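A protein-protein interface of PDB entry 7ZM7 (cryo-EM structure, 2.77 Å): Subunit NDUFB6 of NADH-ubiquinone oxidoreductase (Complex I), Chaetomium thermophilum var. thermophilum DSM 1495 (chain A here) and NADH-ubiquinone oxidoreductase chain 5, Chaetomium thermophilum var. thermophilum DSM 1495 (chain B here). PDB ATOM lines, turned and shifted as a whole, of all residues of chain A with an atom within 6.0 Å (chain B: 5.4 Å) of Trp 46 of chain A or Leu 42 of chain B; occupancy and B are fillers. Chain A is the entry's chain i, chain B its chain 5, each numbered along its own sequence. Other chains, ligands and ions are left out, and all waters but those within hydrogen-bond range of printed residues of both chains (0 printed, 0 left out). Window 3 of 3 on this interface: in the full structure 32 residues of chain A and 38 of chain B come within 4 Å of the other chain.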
ATOM      1  N   ILE A  41     -19.138 -11.240 -14.712  1.00  0.00           N
ATOM      2  CA  ILE A  41     -19.112 -10.039 -13.823  1.00  0.00           C
ATOM      3  C   ILE A  41     -20.349  -9.183 -14.110  1.00  0.00           C
ATOM      4  O   ILE A  41     -20.994  -8.743 -13.146  1.00  0.00           O
ATOM      5  CB  ILE A  41     -17.806  -9.240 -14.006  1.00  0.00           C
ATOM      6  CG1 ILE A  41     -16.588 -10.019 -13.503  1.00  0.00           C
ATOM      7  CG2 ILE A  41     -17.901  -7.877 -13.339  1.00  0.00           C
ATOM      8  CD1 ILE A  41     -15.271  -9.356 -13.820  1.00  0.00           C
ATOM      9  N   THR A  42     -20.691  -9.005 -15.386  1.00  0.00           N
ATOM     10  CA  THR A  42     -21.868  -8.179 -15.766  1.00  0.00           C
ATOM     11  C   THR A  42     -23.144  -8.831 -15.218  1.00  0.00           C
ATOM     12  O   THR A  42     -24.039  -8.086 -14.792  1.00  0.00           O
ATOM     13  CB  THR A  42     -21.866  -7.828 -17.261  1.00  0.00           C
ATOM     14  OG1 THR A  42     -22.581  -6.600 -17.407  1.00  0.00           O
ATOM     15  CG2 THR A  42     -22.492  -8.886 -18.142  1.00  0.00           C
ATOM     16  N   ALA A  43     -23.215 -10.166 -15.245  1.00  0.00           N
ATOM     17  CA  ALA A  43     -24.394 -10.908 -14.743  1.00  0.00           C
ATOM     18  C   ALA A  43     -24.572 -10.658 -13.243  1.00  0.00           C
ATOM     19  O   ALA A  43     -25.723 -10.475 -12.809  1.00  0.00           O
ATOM     20  CB  ALA A  43     -24.233 -12.379 -15.036  1.00  0.00           C
ATOM     21  N   MET A  44     -23.474 -10.653 -12.484  1.00  0.00           N
ATOM     22  CA  MET A  44     -23.556 -10.348 -11.033  1.00  0.00           C
ATOM     23  C   MET A  44     -24.052  -8.912 -10.851  1.00  0.00           C
ATOM     24  O   MET A  44     -24.894  -8.687  -9.964  1.00  0.00           O
ATOM     25  CB  MET A  44     -22.180 -10.479 -10.376  1.00  0.00           C
ATOM     26  CG  MET A  44     -21.658 -11.901 -10.337  1.00  0.00           C
ATOM     27  SD  MET A  44     -20.028 -11.983  -9.557  1.00  0.00           S
ATOM     28  CE  MET A  44     -20.336 -11.027  -8.073  1.00  0.00           C
ATOM     29  N   VAL A  45     -23.553  -7.986 -11.674  1.00  0.00           N
ATOM     30  CA  VAL A  45     -23.937  -6.551 -11.556  1.00  0.00           C
ATOM     31  C   VAL A  45     -25.409  -6.390 -11.954  1.00  0.00           C
ATOM     32  O   VAL A  45     -26.086  -5.542 -11.350  1.00  0.00           O
ATOM     33  CB  VAL A  45     -22.989  -5.655 -12.380  1.00  0.00           C
ATOM     34  CG1 VAL A  45     -23.417  -4.198 -12.353  1.00  0.00           C
ATOM     35  CG2 VAL A  45     -21.552  -5.785 -11.906  1.00  0.00           C
ATOM     36  N   TRP A  46     -25.891  -7.183 -12.917  1.00  0.00           N
ATOM     37  CA  TRP A  46     -27.293  -7.114 -13.313  1.00  0.00           C
ATOM     38  C   TRP A  46     -28.214  -7.631 -12.219  1.00  0.00           C
ATOM     39  O   TRP A  46     -29.248  -7.022 -11.930  1.00  0.00           O
ATOM     40  CB  TRP A  46     -27.498  -7.900 -14.601  1.00  0.00           C
ATOM     41  CG  TRP A  46     -28.749  -7.591 -15.344  1.00  0.00           C
ATOM     42  CD1 TRP A  46     -30.016  -7.807 -14.926  1.00  0.00           C
ATOM     43  CD2 TRP A  46     -28.848  -7.024 -16.649  1.00  0.00           C
ATOM     44  NE1 TRP A  46     -30.902  -7.414 -15.881  1.00  0.00           N
ATOM     45  CE2 TRP A  46     -30.212  -6.930 -16.953  1.00  0.00           C
ATOM     46  CE3 TRP A  46     -27.915  -6.581 -17.586  1.00  0.00           C
ATOM     47  CZ2 TRP A  46     -30.673  -6.412 -18.148  1.00  0.00           C
ATOM     48  CZ3 TRP A  46     -28.371  -6.073 -18.774  1.00  0.00           C
ATOM     49  CH2 TRP A  46     -29.739  -5.988 -19.047  1.00  0.00           C
ATOM     50  N   LYS A  47     -27.860  -8.755 -11.599  1.00  0.00           N
ATOM     51  CA  LYS A  47     -28.668  -9.250 -10.497  1.00  0.00           C
ATOM     52  C   LYS A  47     -28.641  -8.281  -9.329  1.00  0.00           C
ATOM     53  O   LYS A  47     -29.612  -8.185  -8.573  1.00  0.00           O
ATOM     54  CB  LYS A  47     -28.183 -10.628 -10.060  1.00  0.00           C
ATOM     55  CG  LYS A  47     -29.041 -11.265  -8.984  1.00  0.00           C
ATOM     56  CD  LYS A  47     -28.572 -12.662  -8.641  1.00  0.00           C
ATOM     57  CE  LYS A  47     -29.442 -13.273  -7.558  1.00  0.00           C
ATOM     58  NZ  LYS A  47     -29.005 -14.647  -7.195  1.00  0.00           N
ATOM     59  N   TYR A  48     -27.535  -7.555  -9.158  1.00  0.00           N
ATOM     60  CA  TYR A  48     -27.506  -6.509  -8.145  1.00  0.00           C
ATOM     61  C   TYR A  48     -28.505  -5.404  -8.464  1.00  0.00           C
ATOM     62  O   TYR A  48     -29.310  -5.030  -7.608  1.00  0.00           O
ATOM     63  CB  TYR A  48     -26.112  -5.921  -8.009  1.00  0.00           C
ATOM     64  CG  TYR A  48     -26.047  -4.883  -6.920  1.00  0.00           C
ATOM     65  CD1 TYR A  48     -25.895  -5.247  -5.602  1.00  0.00           C
ATOM     66  CD2 TYR A  48     -26.199  -3.548  -7.209  1.00  0.00           C
ATOM     67  CE1 TYR A  48     -25.856  -4.313  -4.619  1.00  0.00           C
ATOM     68  CE2 TYR A  48     -26.176  -2.610  -6.226  1.00  0.00           C
ATOM     69  CZ  TYR A  48     -26.003  -2.995  -4.932  1.00  0.00           C
ATOM     70  OH  TYR A  48     -25.970  -2.045  -3.937  1.00  0.00           O
ATOM     71  N   SER A  49     -28.480  -4.879  -9.693  1.00  0.00           N
ATOM     72  CA  SER A  49     -29.386  -3.795 -10.054  1.00  0.00           C
ATOM     73  C   SER A  49     -30.835  -4.212  -9.895  1.00  0.00           C
ATOM     74  O   SER A  49     -31.633  -3.492  -9.291  1.00  0.00           O
ATOM     75  CB  SER A  49     -29.148  -3.367 -11.495  1.00  0.00           C
ATOM     76  OG  SER A  49     -27.780  -3.169 -11.754  1.00  0.00           O
ATOM     77  N   ALA A  50     -31.178  -5.398 -10.396  1.00  0.00           N
ATOM     78  CA  ALA A  50     -32.548  -5.878 -10.349  1.00  0.00           C
ATOM     79  C   ALA A  50     -33.114  -5.789  -8.947  1.00  0.00           C
ATOM     80  O   ALA A  50     -34.283  -5.440  -8.759  1.00  0.00           O
ATOM     81  CB  ALA A  50     -32.594  -7.319 -10.839  1.00  0.00           C
ATOM     82  N   GLU A  51     -32.286  -6.071  -7.950  1.00  0.00           N
ATOM     83  CA  GLU A  51     -32.707  -6.137  -6.561  1.00  0.00           C
ATOM     84  C   GLU A  51     -32.451  -4.860  -5.781  1.00  0.00           C
ATOM     85  O   GLU A  51     -32.745  -4.823  -4.586  1.00  0.00           O
ATOM     86  CB  GLU A  51     -32.000  -7.296  -5.864  1.00  0.00           C
ATOM     87  CG  GLU A  51     -32.415  -8.661  -6.351  1.00  0.00           C
ATOM     88  CD  GLU A  51     -31.962  -9.770  -5.416  1.00  0.00           C
ATOM     89  OE1 GLU A  51     -32.832 -10.417  -4.796  1.00  0.00           O
ATOM     90  OE2 GLU A  51     -30.738  -9.989  -5.294  1.00  0.00           O
ATOM     91  N   TRP A  70     -37.216  -8.249 -14.880  1.00  0.00           N
ATOM     92  CA  TRP A  70     -36.103  -8.665 -13.989  1.00  0.00           C
ATOM     93  C   TRP A  70     -36.028  -7.859 -12.694  1.00  0.00           C
ATOM     94  O   TRP A  70     -35.255  -8.268 -11.828  1.00  0.00           O
ATOM     95  CB  TRP A  70     -34.754  -8.674 -14.719  1.00  0.00           C
ATOM     96  CG  TRP A  70     -34.451  -7.428 -15.491  1.00  0.00           C
ATOM     97  CD1 TRP A  70     -33.997  -6.239 -14.998  1.00  0.00           C
ATOM     98  CD2 TRP A  70     -34.561  -7.254 -16.912  1.00  0.00           C
ATOM     99  NE1 TRP A  70     -33.830  -5.337 -16.011  1.00  0.00           N
ATOM    100  CE2 TRP A  70     -34.164  -5.932 -17.198  1.00  0.00           C
ATOM    101  CE3 TRP A  70     -34.954  -8.083 -17.967  1.00  0.00           C
ATOM    102  CZ2 TRP A  70     -34.153  -5.424 -18.494  1.00  0.00           C
ATOM    103  CZ3 TRP A  70     -34.941  -7.581 -19.248  1.00  0.00           C
ATOM    104  CH2 TRP A  70     -34.543  -6.270 -19.505  1.00  0.00           C
ATOM    105  N   MET B   1     -29.551  -3.586 -15.036  1.00  0.00           N
ATOM    106  CA  MET B   1     -29.429  -3.023 -16.371  1.00  0.00           C
ATOM    107  C   MET B   1     -28.794  -1.657 -16.308  1.00  0.00           C
ATOM    108  O   MET B   1     -27.828  -1.371 -17.006  1.00  0.00           O
ATOM    109  CB  MET B   1     -30.788  -2.922 -17.059  1.00  0.00           C
ATOM    110  CG  MET B   1     -30.678  -2.533 -18.516  1.00  0.00           C
ATOM    111  SD  MET B   1     -31.961  -1.457 -19.183  1.00  0.00           S
ATOM    112  CE  MET B   1     -31.355   0.145 -18.703  1.00  0.00           C
ATOM    113  N   SER B   4     -25.541  -1.893 -15.133  1.00  0.00           N
ATOM    114  CA  SER B   4     -24.737  -2.587 -16.130  1.00  0.00           C
ATOM    115  C   SER B   4     -24.278  -1.654 -17.235  1.00  0.00           C
ATOM    116  O   SER B   4     -23.221  -1.880 -17.828  1.00  0.00           O
ATOM    117  CB  SER B   4     -25.514  -3.758 -16.734  1.00  0.00           C
ATOM    118  OG  SER B   4     -25.737  -4.777 -15.778  1.00  0.00           O
ATOM    119  N   ILE B   5     -25.054  -0.612 -17.527  1.00  0.00           N
ATOM    120  CA  ILE B   5     -24.593   0.405 -18.468  1.00  0.00           C
ATOM    121  C   ILE B   5     -23.297   1.017 -17.973  1.00  0.00           C
ATOM    122  O   ILE B   5     -22.362   1.255 -18.740  1.00  0.00           O
ATOM    123  CB  ILE B   5     -25.677   1.479 -18.666  1.00  0.00           C
ATOM    124  CG1 ILE B   5     -26.812   0.936 -19.511  1.00  0.00           C
ATOM    125  CG2 ILE B   5     -25.090   2.711 -19.313  1.00  0.00           C
ATOM    126  CD1 ILE B   5     -27.955   1.894 -19.630  1.00  0.00           C
ATOM    127  N   LEU B   8     -20.033  -1.974 -18.134  1.00  0.00           N
ATOM    128  CA  LEU B   8     -19.471  -2.580 -19.341  1.00  0.00           C
ATOM    129  C   LEU B   8     -18.343  -1.785 -19.964  1.00  0.00           C
ATOM    130  O   LEU B   8     -17.308  -2.387 -20.290  1.00  0.00           O
ATOM    131  CB  LEU B   8     -20.565  -2.842 -20.376  1.00  0.00           C
ATOM    132  CG  LEU B   8     -21.632  -3.872 -20.091  1.00  0.00           C
ATOM    133  CD1 LEU B   8     -22.659  -3.851 -21.163  1.00  0.00           C
ATOM    134  CD2 LEU B   8     -20.933  -5.177 -20.147  1.00  0.00           C
ATOM    135  N   ILE B  38     -22.697  -3.109 -26.751  1.00  0.00           N
ATOM    136  CA  ILE B  38     -23.740  -3.650 -25.879  1.00  0.00           C
ATOM    137  C   ILE B  38     -24.305  -2.564 -24.977  1.00  0.00           C
ATOM    138  O   ILE B  38     -25.518  -2.492 -24.755  1.00  0.00           O
ATOM    139  CB  ILE B  38     -23.185  -4.820 -25.050  1.00  0.00           C
ATOM    140  CG1 ILE B  38     -22.752  -5.970 -25.949  1.00  0.00           C
ATOM    141  CG2 ILE B  38     -24.219  -5.324 -24.089  1.00  0.00           C
ATOM    142  CD1 ILE B  38     -21.962  -7.034 -25.219  1.00  0.00           C
ATOM    143  N   THR B  39     -23.430  -1.718 -24.425  1.00  0.00           N
ATOM    144  CA  THR B  39     -23.875  -0.650 -23.540  1.00  0.00           C
ATOM    145  C   THR B  39     -24.812   0.301 -24.258  1.00  0.00           C
ATOM    146  O   THR B  39     -25.740   0.845 -23.654  1.00  0.00           O
ATOM    147  CB  THR B  39     -22.663   0.106 -22.995  1.00  0.00           C
ATOM    148  OG1 THR B  39     -21.634  -0.823 -22.651  1.00  0.00           O
ATOM    149  CG2 THR B  39     -23.028   0.909 -21.780  1.00  0.00           C
ATOM    150  N   THR B  40     -24.587   0.494 -25.552  1.00  0.00           N
ATOM    151  CA  THR B  40     -25.387   1.413 -26.346  1.00  0.00           C
ATOM    152  C   THR B  40     -26.823   0.924 -26.510  1.00  0.00           C
ATOM    153  O   THR B  40     -27.758   1.726 -26.441  1.00  0.00           O
ATOM    154  CB  THR B  40     -24.710   1.603 -27.691  1.00  0.00           C
ATOM    155  OG1 THR B  40     -23.309   1.734 -27.460  1.00  0.00           O
ATOM    156  CG2 THR B  40     -25.226   2.842 -28.379  1.00  0.00           C
ATOM    157  N   ILE B  41     -27.026  -0.375 -26.740  1.00  0.00           N
ATOM    158  CA  ILE B  41     -28.391  -0.884 -26.807  1.00  0.00           C
ATOM    159  C   ILE B  41     -29.077  -0.747 -25.459  1.00  0.00           C
ATOM    160  O   ILE B  41     -30.237  -0.327 -25.378  1.00  0.00           O
ATOM    161  CB  ILE B  41     -28.425  -2.341 -27.307  1.00  0.00           C
ATOM    162  CG1 ILE B  41     -27.880  -2.462 -28.730  1.00  0.00           C
ATOM    163  CG2 ILE B  41     -29.837  -2.901 -27.235  1.00  0.00           C
ATOM    164  CD1 ILE B  41     -26.472  -2.952 -28.807  1.00  0.00           C
ATOM    165  N   LEU B  42     -28.368  -1.086 -24.378  1.00  0.00           N
ATOM    166  CA  LEU B  42     -28.921  -0.964 -23.036  1.00  0.00           C
ATOM    167  C   LEU B  42     -29.400   0.444 -22.745  1.00  0.00           C
ATOM    168  O   LEU B  42     -30.294   0.633 -21.918  1.00  0.00           O
ATOM    169  CB  LEU B  42     -27.873  -1.354 -22.001  1.00  0.00           C
ATOM    170  CG  LEU B  42     -27.361  -2.776 -21.910  1.00  0.00           C
ATOM    171  CD1 LEU B  42     -26.242  -2.820 -20.903  1.00  0.00           C
ATOM    172  CD2 LEU B  42     -28.491  -3.697 -21.494  1.00  0.00           C
ATOM    173  N   SER B  43     -28.789   1.445 -23.374  1.00  0.00           N
ATOM    174  CA  SER B  43     -29.136   2.834 -23.112  1.00  0.00           C
ATOM    175  C   SER B  43     -30.194   3.364 -24.059  1.00  0.00           C
ATOM    176  O   SER B  43     -30.942   4.278 -23.696  1.00  0.00           O
ATOM    177  CB  SER B  43     -27.891   3.700 -23.201  1.00  0.00           C
ATOM    178  OG  SER B  43     -26.958   3.288 -22.239  1.00  0.00           O
ATOM    179  N   ILE B  44     -30.259   2.822 -25.271  1.00  0.00           N
ATOM    180  CA  ILE B  44     -31.426   3.043 -26.109  1.00  0.00           C
ATOM    181  C   ILE B  44     -32.668   2.535 -25.397  1.00  0.00           C
ATOM    182  O   ILE B  44     -33.723   3.179 -25.417  1.00  0.00           O
ATOM    183  CB  ILE B  44     -31.240   2.362 -27.476  1.00  0.00           C
ATOM    184  CG1 ILE B  44     -30.032   2.945 -28.208  1.00  0.00           C
ATOM    185  CG2 ILE B  44     -32.490   2.496 -28.311  1.00  0.00           C
ATOM    186  CD1 ILE B  44     -30.178   4.382 -28.562  1.00  0.00           C
ATOM    187  N   ILE B  45     -32.561   1.374 -24.753  1.00  0.00           N
ATOM    188  CA  ILE B  45     -33.689   0.828 -24.016  1.00  0.00           C
ATOM    189  C   ILE B  45     -34.028   1.719 -22.836  1.00  0.00           C
ATOM    190  O   ILE B  45     -35.201   2.012 -22.578  1.00  0.00           O
ATOM    191  CB  ILE B  45     -33.389  -0.612 -23.570  1.00  0.00           C
ATOM    192  CG1 ILE B  45     -33.104  -1.500 -24.781  1.00  0.00           C
ATOM    193  CG2 ILE B  45     -34.550  -1.176 -22.785  1.00  0.00           C
ATOM    194  CD1 ILE B  45     -34.261  -1.597 -25.747  1.00  0.00           C
ATOM    195  N   ALA B  46     -33.004   2.182 -22.113  1.00  0.00           N
ATOM    196  CA  ALA B  46     -33.227   3.031 -20.949  1.00  0.00           C
ATOM    197  C   ALA B  46     -33.877   4.353 -21.321  1.00  0.00           C
ATOM    198  O   ALA B  46     -34.502   4.991 -20.473  1.00  0.00           O
ATOM    199  CB  ALA B  46     -31.912   3.281 -20.224  1.00  0.00           C
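Of the printed residues of chain B, Trp 46 of chain A touches Met 1 (3.6 Å), Ser 4 (3.4 Å) and Leu 42 (3.6 Å). Of the printed residues of chain B, Ser 49 of chain A touches Met 1. Printed residues of chain A within 4 Å of Ser 4 of chain B: Thr 42 and Trp 46. Printed residues of chain A within 4 Å of Leu 8 of chain B: Thr 42 (3.5 Å). Ile 41 of chain B touches none of the printed residues of chain A. Leu 42 of chain B touches just one residue of chain A: Trp 46. Ser 43 of chain B touches none of the printed residues of chain A. The nearest printed residue of chain A that does not touch Leu 42 of chain B is Thr 42 of chain A (6.3 Å).
O of Thr 42 of chain A touches OG of Ser 4 of chain B, 3.8 Å away. Thr 42 of chain A touches Leu 8 of chain B (OG1 to CD2, 3.5 Å). CH2 of Trp 46 of chain A touches CG of Met 1 of chain B, 3.6 Å away. OG of Ser 4 of chain B touches CE3 of Trp 46 of chain A, at 3.4 Å. CH2 of Trp 46 of chain A touches CD2 of Leu 42 of chain B, 3.6 Å away. Ser 49 of chain A touches Met 1 of chain B (CB to N, 3.6 Å).
O of Val 45 of chain A is in hydrogen-bond range of OG of Ser 49 of chain A (2.9 Å).
Of the 12 printed residues of chain A, 3 touch a printed residue of chain B. Hydrophobic or aromatic side chains of chain A that line the printed part of chain B: Trp 46. Along chain A the printed residues that touch a printed residue of chain B span positions 42 to 49. Of the 13 printed residues of chain B, 4 touch a printed residue of chain A. Hydrophobic or aromatic side chains of chain B that line the printed part of chain A: Met 1, Leu 8 and Leu 42. Along chain B the printed residues that touch a printed residue of chain A span positions 1 to 42. Among the printed residues, 6 pairs touch across the chains.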
